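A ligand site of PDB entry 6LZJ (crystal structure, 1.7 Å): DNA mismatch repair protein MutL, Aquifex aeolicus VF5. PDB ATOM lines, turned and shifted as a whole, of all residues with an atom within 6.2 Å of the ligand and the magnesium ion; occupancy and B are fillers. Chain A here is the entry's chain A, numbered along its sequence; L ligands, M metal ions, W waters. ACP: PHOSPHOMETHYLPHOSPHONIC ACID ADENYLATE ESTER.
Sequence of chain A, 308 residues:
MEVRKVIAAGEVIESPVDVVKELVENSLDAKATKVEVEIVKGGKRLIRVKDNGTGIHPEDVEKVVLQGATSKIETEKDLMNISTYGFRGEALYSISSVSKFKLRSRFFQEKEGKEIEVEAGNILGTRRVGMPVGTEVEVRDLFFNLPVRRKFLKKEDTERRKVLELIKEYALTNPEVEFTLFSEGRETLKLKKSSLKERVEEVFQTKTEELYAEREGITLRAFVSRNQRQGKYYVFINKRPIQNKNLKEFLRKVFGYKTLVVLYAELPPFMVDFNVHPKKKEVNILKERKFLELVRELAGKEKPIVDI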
ATOM      1  N   GLU A  22      10.491 -11.173  19.145  1.00  0.00           N
ATOM      2  CA  GLU A  22      10.481  -9.812  18.628  1.00  0.00           C
ATOM      3  C   GLU A  22      11.787  -9.118  18.929  1.00  0.00           C
ATOM      4  O   GLU A  22      12.338  -8.412  18.072  1.00  0.00           O
ATOM      5  CB  GLU A  22       9.310  -9.033  19.251  1.00  0.00           C
ATOM      6  CG  GLU A  22       7.902  -9.472  18.728  1.00  0.00           C
ATOM      7  CD  GLU A  22       7.696  -9.398  17.235  1.00  0.00           C
ATOM      8  OE1 GLU A  22       8.364  -8.593  16.538  1.00  0.00           O
ATOM      9  OE2 GLU A  22       6.847 -10.186  16.748  1.00  0.00           O
ATOM     10  N   LEU A  23      12.323  -9.346  20.131  1.00  0.00           N
ATOM     11  CA  LEU A  23      13.579  -8.687  20.426  1.00  0.00           C
ATOM     12  C   LEU A  23      14.716  -9.237  19.582  1.00  0.00           C
ATOM     13  O   LEU A  23      15.553  -8.471  19.094  1.00  0.00           O
ATOM     14  CB  LEU A  23      13.873  -8.861  21.905  1.00  0.00           C
ATOM     15  CG  LEU A  23      12.808  -8.141  22.727  1.00  0.00           C
ATOM     16  CD1 LEU A  23      13.195  -8.289  24.216  1.00  0.00           C
ATOM     17  CD2 LEU A  23      12.663  -6.666  22.409  1.00  0.00           C
ATOM     18  N   GLU A  25      14.590 -10.694  16.676  1.00  0.00           N
ATOM     19  CA  GLU A  25      14.434 -10.186  15.306  1.00  0.00           C
ATOM     20  C   GLU A  25      15.019  -8.786  15.173  1.00  0.00           C
ATOM     21  O   GLU A  25      15.760  -8.491  14.208  1.00  0.00           O
ATOM     22  CB  GLU A  25      12.948 -10.199  14.912  1.00  0.00           C
ATOM     23  CG  GLU A  25      12.715  -9.714  13.485  1.00  0.00           C
ATOM     24  CD  GLU A  25      11.264  -9.835  13.080  1.00  0.00           C
ATOM     25  OE1 GLU A  25      10.549  -8.792  12.969  1.00  0.00           O
ATOM     26  OE2 GLU A  25      10.839 -10.978  12.902  1.00  0.00           O
ATOM     27  N   ASN A  26      14.643  -7.911  16.091  1.00  0.00           N
ATOM     28  CA  ASN A  26      15.158  -6.527  16.123  1.00  0.00           C
ATOM     29  C   ASN A  26      16.679  -6.490  16.185  1.00  0.00           C
ATOM     30  O   ASN A  26      17.330  -5.691  15.492  1.00  0.00           O
ATOM     31  CB  ASN A  26      14.557  -5.794  17.320  1.00  0.00           C
ATOM     32  CG  ASN A  26      13.129  -5.363  17.114  1.00  0.00           C
ATOM     33  OD1 ASN A  26      12.447  -4.938  18.054  1.00  0.00           O
ATOM     34  ND2 ASN A  26      12.656  -5.449  15.871  1.00  0.00           N
ATOM     35  N   SER A  27      17.271  -7.367  16.971  1.00  0.00           N
ATOM     36  CA  SER A  27      18.725  -7.407  17.015  1.00  0.00           C
ATOM     37  C   SER A  27      19.301  -7.816  15.679  1.00  0.00           C
ATOM     38  O   SER A  27      20.261  -7.204  15.210  1.00  0.00           O
ATOM     39  CB  SER A  27      19.177  -8.378  18.094  1.00  0.00           C
ATOM     40  OG  SER A  27      18.621  -7.958  19.326  1.00  0.00           O
ATOM     41  N   ASP A  29      17.881  -7.536  12.761  1.00  0.00           N
ATOM     42  CA  ASP A  29      17.598  -6.413  11.864  1.00  0.00           C
ATOM     43  C   ASP A  29      18.650  -5.324  11.996  1.00  0.00           C
ATOM     44  O   ASP A  29      18.929  -4.604  11.037  1.00  0.00           O
ATOM     45  CB  ASP A  29      16.235  -5.792  12.173  1.00  0.00           C
ATOM     46  CG  ASP A  29      15.052  -6.648  11.709  1.00  0.00           C
ATOM     47  OD1 ASP A  29      15.232  -7.629  10.936  1.00  0.00           O
ATOM     48  OD2 ASP A  29      13.933  -6.329  12.193  1.00  0.00           O
ATOM     49  N   ALA A  30      19.214  -5.175  13.187  1.00  0.00           N
ATOM     50  CA  ALA A  30      20.214  -4.165  13.478  1.00  0.00           C
ATOM     51  C   ALA A  30      21.648  -4.649  13.240  1.00  0.00           C
ATOM     52  O   ALA A  30      22.591  -4.045  13.764  1.00  0.00           O
ATOM     53  CB  ALA A  30      20.054  -3.679  14.905  1.00  0.00           C
ATOM     54  N   ASP A  51      22.383  -6.981  22.434  1.00  0.00           N
ATOM     55  CA  ASP A  51      23.039  -7.183  21.162  1.00  0.00           C
ATOM     56  C   ASP A  51      24.128  -6.147  20.980  1.00  0.00           C
ATOM     57  O   ASP A  51      24.199  -5.109  21.668  1.00  0.00           O
ATOM     58  CB  ASP A  51      22.004  -7.155  19.968  1.00  0.00           C
ATOM     59  CG  ASP A  51      21.398  -5.797  19.740  1.00  0.00           C
ATOM     60  OD1 ASP A  51      22.179  -4.847  19.481  1.00  0.00           O
ATOM     61  OD2 ASP A  51      20.174  -5.685  19.789  1.00  0.00           O
ATOM     62  N   GLY A  53      24.566  -4.782  17.833  1.00  0.00           N
ATOM     63  CA  GLY A  53      24.277  -4.066  16.608  1.00  0.00           C
ATOM     64  C   GLY A  53      24.460  -2.555  16.693  1.00  0.00           C
ATOM     65  O   GLY A  53      24.992  -2.032  17.675  1.00  0.00           O
ATOM     66  N   THR A  54      23.976  -1.837  15.675  1.00  0.00           N
ATOM     67  CA  THR A  54      24.327  -0.425  15.504  1.00  0.00           C
ATOM     68  C   THR A  54      23.676   0.501  16.510  1.00  0.00           C
ATOM     69  O   THR A  54      24.009   1.690  16.536  1.00  0.00           O
ATOM     70  CB  THR A  54      23.972   0.022  14.086  1.00  0.00           C
ATOM     71  OG1 THR A  54      22.656  -0.451  13.739  1.00  0.00           O
ATOM     72  CG2 THR A  54      24.982  -0.542  13.108  1.00  0.00           C
ATOM     73  N   GLY A  55      22.741   0.006  17.326  1.00  0.00           N
ATOM     74  CA  GLY A  55      22.057   0.823  18.298  1.00  0.00           C
ATOM     75  C   GLY A  55      21.045   1.787  17.718  1.00  0.00           C
ATOM     76  O   GLY A  55      20.748   1.819  16.523  1.00  0.00           O
ATOM     77  N   ILE A  56      20.510   2.594  18.622  1.00  0.00           N
ATOM     78  CA  ILE A  56      19.485   3.584  18.328  1.00  0.00           C
ATOM     79  C   ILE A  56      20.032   4.933  18.757  1.00  0.00           C
ATOM     80  O   ILE A  56      20.564   5.044  19.865  1.00  0.00           O
ATOM     81  CB  ILE A  56      18.161   3.255  19.050  1.00  0.00           C
ATOM     82  CG1 ILE A  56      17.742   1.805  18.779  1.00  0.00           C
ATOM     83  CG2 ILE A  56      17.048   4.180  18.620  1.00  0.00           C
ATOM     84  CD1 ILE A  56      16.813   1.210  19.849  1.00  0.00           C
ATOM     85  N   LYS A  63      11.051   7.522  20.570  1.00  0.00           N
ATOM     86  CA  LYS A  63      10.120   7.247  19.479  1.00  0.00           C
ATOM     87  C   LYS A  63       9.753   5.765  19.412  1.00  0.00           C
ATOM     88  O   LYS A  63       8.567   5.409  19.339  1.00  0.00           O
ATOM     89  CB  LYS A  63      10.720   7.728  18.168  1.00  0.00           C
ATOM     90  CG  LYS A  63       9.929   7.373  16.907  1.00  0.00           C
ATOM     91  CD  LYS A  63      10.397   6.053  16.291  1.00  0.00           C
ATOM     92  CE  LYS A  63       9.760   5.776  14.944  1.00  0.00           C
ATOM     93  NZ  LYS A  63      10.056   4.379  14.490  1.00  0.00           N
ATOM     94  N   VAL A  64      10.755   4.881  19.412  1.00  0.00           N
ATOM     95  CA  VAL A  64      10.491   3.491  19.053  1.00  0.00           C
ATOM     96  C   VAL A  64       9.662   2.762  20.096  1.00  0.00           C
ATOM     97  O   VAL A  64       9.244   1.634  19.853  1.00  0.00           O
ATOM     98  CB  VAL A  64      11.808   2.764  18.748  1.00  0.00           C
ATOM     99  CG1 VAL A  64      12.498   3.410  17.563  1.00  0.00           C
ATOM    100  CG2 VAL A  64      12.738   2.762  19.943  1.00  0.00           C
ATOM    101  N   GLU A  90       3.409  -1.064  16.978  1.00  0.00           N
ATOM    102  CA  GLU A  90       4.538  -1.889  16.571  1.00  0.00           C
ATOM    103  C   GLU A  90       4.968  -2.778  17.738  1.00  0.00           C
ATOM    104  O   GLU A  90       4.342  -2.768  18.793  1.00  0.00           O
ATOM    105  CB  GLU A  90       5.699  -1.028  16.093  1.00  0.00           C
ATOM    106  CG  GLU A  90       5.472  -0.361  14.752  1.00  0.00           C
ATOM    107  CD  GLU A  90       5.903  -1.228  13.577  1.00  0.00           C
ATOM    108  OE1 GLU A  90       5.722  -2.463  13.656  1.00  0.00           O
ATOM    109  OE2 GLU A  90       6.430  -0.678  12.596  1.00  0.00           O
ATOM    110  N   ALA A  91       6.031  -3.535  17.528  1.00  0.00           N
ATOM    111  CA  ALA A  91       6.345  -4.617  18.443  1.00  0.00           C
ATOM    112  C   ALA A  91       6.766  -4.088  19.824  1.00  0.00           C
ATOM    113  O   ALA A  91       6.278  -4.592  20.843  1.00  0.00           O
ATOM    114  CB  ALA A  91       7.424  -5.528  17.855  1.00  0.00           C
ATOM    115  N   LEU A  92       7.643  -3.070  19.881  1.00  0.00           N
ATOM    116  CA  LEU A  92       8.130  -2.641  21.201  1.00  0.00           C
ATOM    117  C   LEU A  92       7.035  -1.985  22.027  1.00  0.00           C
ATOM    118  O   LEU A  92       6.958  -2.187  23.256  1.00  0.00           O
ATOM    119  CB  LEU A  92       9.308  -1.685  21.048  1.00  0.00           C
ATOM    120  CG  LEU A  92      10.619  -2.390  20.653  1.00  0.00           C
ATOM    121  CD1 LEU A  92      11.736  -1.346  20.567  1.00  0.00           C
ATOM    122  CD2 LEU A  92      11.000  -3.536  21.616  1.00  0.00           C
ATOM    123  N   TYR A  93       6.183  -1.208  21.355  1.00  0.00           N
ATOM    124  CA  TYR A  93       5.031  -0.598  22.018  1.00  0.00           C
ATOM    125  C   TYR A  93       4.146  -1.677  22.617  1.00  0.00           C
ATOM    126  O   TYR A  93       3.716  -1.591  23.772  1.00  0.00           O
ATOM    127  CB  TYR A  93       4.244   0.242  21.031  1.00  0.00           C
ATOM    128  CG  TYR A  93       2.947   0.753  21.618  1.00  0.00           C
ATOM    129  CD1 TYR A  93       2.947   1.722  22.614  1.00  0.00           C
ATOM    130  CD2 TYR A  93       1.731   0.211  21.218  1.00  0.00           C
ATOM    131  CE1 TYR A  93       1.758   2.169  23.169  1.00  0.00           C
ATOM    132  CE2 TYR A  93       0.545   0.664  21.765  1.00  0.00           C
ATOM    133  CZ  TYR A  93       0.566   1.634  22.742  1.00  0.00           C
ATOM    134  OH  TYR A  93      -0.625   2.064  23.282  1.00  0.00           O
ATOM    135  N   LEU A 103      14.514  -0.131  27.864  1.00  0.00           N
ATOM    136  CA  LEU A 103      15.379  -0.297  26.702  1.00  0.00           C
ATOM    137  C   LEU A 103      16.530   0.679  26.852  1.00  0.00           C
ATOM    138  O   LEU A 103      16.299   1.869  27.074  1.00  0.00           O
ATOM    139  CB  LEU A 103      14.630  -0.041  25.401  1.00  0.00           C
ATOM    140  CG  LEU A 103      15.420  -0.011  24.097  1.00  0.00           C
ATOM    141  CD1 LEU A 103      14.480  -0.463  22.949  1.00  0.00           C
ATOM    142  CD2 LEU A 103      15.925   1.373  23.777  1.00  0.00           C
ATOM    143  N   SER A 105      20.135   1.907  24.741  1.00  0.00           N
ATOM    144  CA  SER A 105      20.827   1.758  23.471  1.00  0.00           C
ATOM    145  C   SER A 105      21.905   2.810  23.300  1.00  0.00           C
ATOM    146  O   SER A 105      21.701   3.979  23.646  1.00  0.00           O
ATOM    147  CB  SER A 105      19.850   1.817  22.281  1.00  0.00           C
ATOM    148  OG  SER A 105      20.575   1.421  21.124  1.00  0.00           O
ATOM    149  N   GLY A 134      25.396  -0.845  21.170  1.00  0.00           N
ATOM    150  CA  GLY A 134      24.419  -1.898  20.944  1.00  0.00           C
ATOM    151  C   GLY A 134      23.155  -1.538  21.684  1.00  0.00           C
ATOM    152  O   GLY A 134      22.950  -0.403  22.122  1.00  0.00           O
ATOM    153  N   THR A 135      22.295  -2.533  21.891  1.00  0.00           N
ATOM    154  CA  THR A 135      20.980  -2.313  22.499  1.00  0.00           C
ATOM    155  C   THR A 135      20.729  -3.410  23.501  1.00  0.00           C
ATOM    156  O   THR A 135      21.091  -4.575  23.289  1.00  0.00           O
ATOM    157  CB  THR A 135      19.865  -2.305  21.436  1.00  0.00           C
ATOM    158  OG1 THR A 135      20.111  -1.264  20.519  1.00  0.00           O
ATOM    159  CG2 THR A 135      18.530  -2.114  22.039  1.00  0.00           C
ATOM    160  N   GLU A 136      20.120  -3.043  24.604  1.00  0.00           N
ATOM    161  CA  GLU A 136      19.754  -4.051  25.591  1.00  0.00           C
ATOM    162  C   GLU A 136      18.336  -3.769  26.056  1.00  0.00           C
ATOM    163  O   GLU A 136      18.033  -2.647  26.478  1.00  0.00           O
ATOM    164  CB  GLU A 136      20.744  -4.027  26.760  1.00  0.00           C
ATOM    165  CG  GLU A 136      20.402  -5.095  27.811  1.00  0.00           C
ATOM    166  CD  GLU A 136      21.552  -5.225  28.796  1.00  0.00           C
ATOM    167  OE1 GLU A 136      22.056  -6.346  28.962  1.00  0.00           O
ATOM    168  OE2 GLU A 136      22.007  -4.166  29.289  1.00  0.00           O
ATOM    169  N   VAL A 137      17.456  -4.755  25.943  1.00  0.00           N
ATOM    170  CA  VAL A 137      16.065  -4.590  26.332  1.00  0.00           C
ATOM    171  C   VAL A 137      15.753  -5.551  27.468  1.00  0.00           C
ATOM    172  O   VAL A 137      16.143  -6.728  27.416  1.00  0.00           O
ATOM    173  CB  VAL A 137      15.135  -4.859  25.125  1.00  0.00           C
ATOM    174  CG1 VAL A 137      13.678  -4.516  25.507  1.00  0.00           C
ATOM    175  CG2 VAL A 137      15.628  -4.055  23.901  1.00  0.00           C
HETATM  176  PG  ACP L   1       8.114  -5.224  13.273  1.00  0.00           P
HETATM  177  O1G ACP L   1       8.894  -5.585  14.483  1.00  0.00           O
HETATM  178  O2G ACP L   1       6.545  -5.115  13.639  1.00  0.00           O
HETATM  179  O3G ACP L   1       8.397  -6.206  12.008  1.00  0.00           O
HETATM  180  PB  ACP L   1       9.886  -2.899  13.743  1.00  0.00           P
HETATM  181  O1B ACP L   1      11.033  -3.786  13.893  1.00  0.00           O
HETATM  182  O2B ACP L   1      10.297  -1.644  12.815  1.00  0.00           O
HETATM  183  C3B ACP L   1       8.586  -3.581  12.704  1.00  0.00           C
HETATM  184  PA  ACP L   1       9.764  -2.549  16.544  1.00  0.00           P
HETATM  185  O1A ACP L   1      10.131  -4.018  16.644  1.00  0.00           O
HETATM  186  O2A ACP L   1       8.704  -2.042  17.472  1.00  0.00           O
HETATM  187  O3A ACP L   1       9.215  -2.272  15.043  1.00  0.00           O
HETATM  188  O5' ACP L   1      11.114  -1.691  16.619  1.00  0.00           O
HETATM  189  C5' ACP L   1      10.926  -0.310  16.277  1.00  0.00           C
HETATM  190  C4' ACP L   1      12.237   0.279  15.806  1.00  0.00           C
HETATM  191  O4' ACP L   1      13.165   0.276  16.893  1.00  0.00           O
HETATM  192  C3' ACP L   1      12.934  -0.515  14.724  1.00  0.00           C
HETATM  193  O3' ACP L   1      12.455  -0.147  13.416  1.00  0.00           O
HETATM  194  C2' ACP L   1      14.366  -0.123  14.907  1.00  0.00           C
HETATM  195  O2' ACP L   1      14.573   1.142  14.232  1.00  0.00           O
HETATM  196  C1' ACP L   1      14.480   0.183  16.393  1.00  0.00           C
HETATM  197  N9  ACP L   1      15.082  -0.951  17.115  1.00  0.00           N
HETATM  198  C8  ACP L   1      14.411  -1.758  17.957  1.00  0.00           C
HETATM  199  N7  ACP L   1      15.250  -2.673  18.495  1.00  0.00           N
HETATM  200  C5  ACP L   1      16.466  -2.405  18.009  1.00  0.00           C
HETATM  201  C6  ACP L   1      17.812  -2.970  18.198  1.00  0.00           C
HETATM  202  N6  ACP L   1      17.986  -4.064  19.018  1.00  0.00           N
HETATM  203  N1  ACP L   1      18.816  -2.422  17.529  1.00  0.00           N
HETATM  204  C2  ACP L   1      18.645  -1.346  16.721  1.00  0.00           C
HETATM  205  N3  ACP L   1      17.467  -0.768  16.477  1.00  0.00           N
HETATM  206  C4  ACP L   1      16.359  -1.260  17.119  1.00  0.00           C
HETATM  207 MG    MG M   1      10.763  -5.385  15.196  1.00  0.00          MG
HETATM  208  O   HOH W   1      11.459  -6.594  13.619  1.00  0.00           O
HETATM  209  O   HOH W   2      21.445  -2.524  18.367  1.00  0.00           O
HETATM  210  O   HOH W   3      17.634   1.237  14.368  1.00  0.00           O
HETATM  211  O   HOH W   4       7.885  -8.728  13.697  1.00  0.00           O
HETATM  212  O   HOH W   5       9.257  -1.184  10.116  1.00  0.00           O
HETATM  213  O   HOH W   6      10.378  -6.992  16.602  1.00  0.00           O
HETATM  214  O   HOH W   7      13.648  -3.743  13.173  1.00  0.00           O
HETATM  215  O   HOH W   8      16.485  -6.131  20.527  1.00  0.00           O
HETATM  216  O   HOH W   9      15.925  -3.250  14.623  1.00  0.00           O
HETATM  217  O   HOH W  10       6.597   0.019  18.756  1.00  0.00           O
HETATM  218  O   HOH W  11      12.405   1.874  11.800  1.00  0.00           O
HETATM  219  O   HOH W  12      14.113  -4.478  20.287  1.00  0.00           O
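Water W6 bridges the side-chain carboxylate (OE1) of Glu 22 (2.6 Å) and the side-chain amide oxygen (OD1) of Asn 26 (3.3 Å). Water W1 lies within hydrogen-bond range of OE1 of Glu 25 (2.5 Å), OD2 of Asp 29 (2.9 Å) and O3G of the ligand (3.5 Å). Water W2 lies within hydrogen-bond range of OD1 of Asp 51, N1 of the ligand, OG1 of Thr 135 and N of Gly 55. Water W8 lies within hydrogen-bond range of O of Leu 23 (2.9 Å), N6 of the ligand (3.0 Å) and OG of Ser 27 (3.1 Å). Water W4 lies within hydrogen-bond range of OE1 of Glu 25 (2.8 Å), OE1 of Glu 22 (2.9 Å) and O3G of the ligand (3.1 Å). Water W10 lies within hydrogen-bond range of N of Tyr 93 (2.9 Å), O2A of the ligand (3.2 Å), O of Val 64 (3.3 Å) and N of Leu 92 (3.4 Å).
The backbone carbonyl oxygen of Glu 22 lies close to the side-chain amide oxygen of Asn 26 (3.5 Å). O of Thr 135 lies within hydrogen-bond range of N of Asp 51. The side-chain carboxylate of Asp 51 sits at hydrogen-bond distance from the side-chain hydroxyl of Ser 27, 2.8 Å away. N of Gly 53 sits at hydrogen-bond distance from OD1 of Asp 51, 2.9 Å away. N of Thr 54 is in hydrogen-bond range of O of Ala 30 (3.2 Å). OG of Ser 105 sits at hydrogen-bond distance from OG1 of Thr 135 (2.8 Å). The backbone NH of Ile 56 is in hydrogen-bond range of the side-chain hydroxyl of Ser 105 (2.8 Å). The side-chain hydroxyl of Ser 27 sits at hydrogen-bond distance from the backbone carbonyl oxygen of Leu 23 (3.1 Å).
The side-chain carboxylate (OE1) of Glu 90 lies close to an oxygen (O2G) of the ligand, 2.8 Å away. The backbone NH (N) of Leu 92 is in hydrogen-bond range of an oxygen (O2A) of the ligand (2.8 Å). OD2 of Asp 51 lies within hydrogen-bond range of N6 of the ligand (2.8 Å). The backbone NH of Ala 91 is in hydrogen-bond range of an oxygen (O2A) of the ligand. The side-chain hydroxyl of Thr 135 lies within hydrogen-bond range of a nitrogen (N1) of the ligand (3.5 Å).
The magnesium ion is bound by O1G of the ligand, at 2.0 Å. The side-chain amide nitrogen (ND2) of Asn 26 binds the magnesium ion. The magnesium ion is bound by O1B of the ligand (2.1 Å). O1A of the ligand binds the magnesium ion (2.1 Å). The magnesium ion is bound by water W1, at 2.1 Å. The magnesium ion is bound by water W6, 2.2 Å away. The magnesium ion has six donor atoms within binding distance.
The side-chain carboxylate (OE1) of Glu 25 sits close to an oxygen (O3G) of the ligand, at 3.5 Å. Merely in contact with the ligand: Glu 22 (3.7 Å), Ser 27 (3.95 Å), Ala 30 (3.2 Å), Gly 55 (3.8 Å), Ile 56 (3.5 Å) and Val 64 (3.3 Å). Hydrophobic or aromatic side chains that line the ligand: Ala 30, Ile 56, Val 64, Ala 91 and Leu 92. 13 residues have an atom within 4 Å of the ligand: Glu 22, Glu 25, Asn 26, Ser 27, Ala 30, Asp 51, Gly 55, Ile 56, Val 64, Glu 90, Ala 91, Leu 92 and Thr 135.
One residue has an atom within 4 Å of the magnesium ion: Asn 26.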
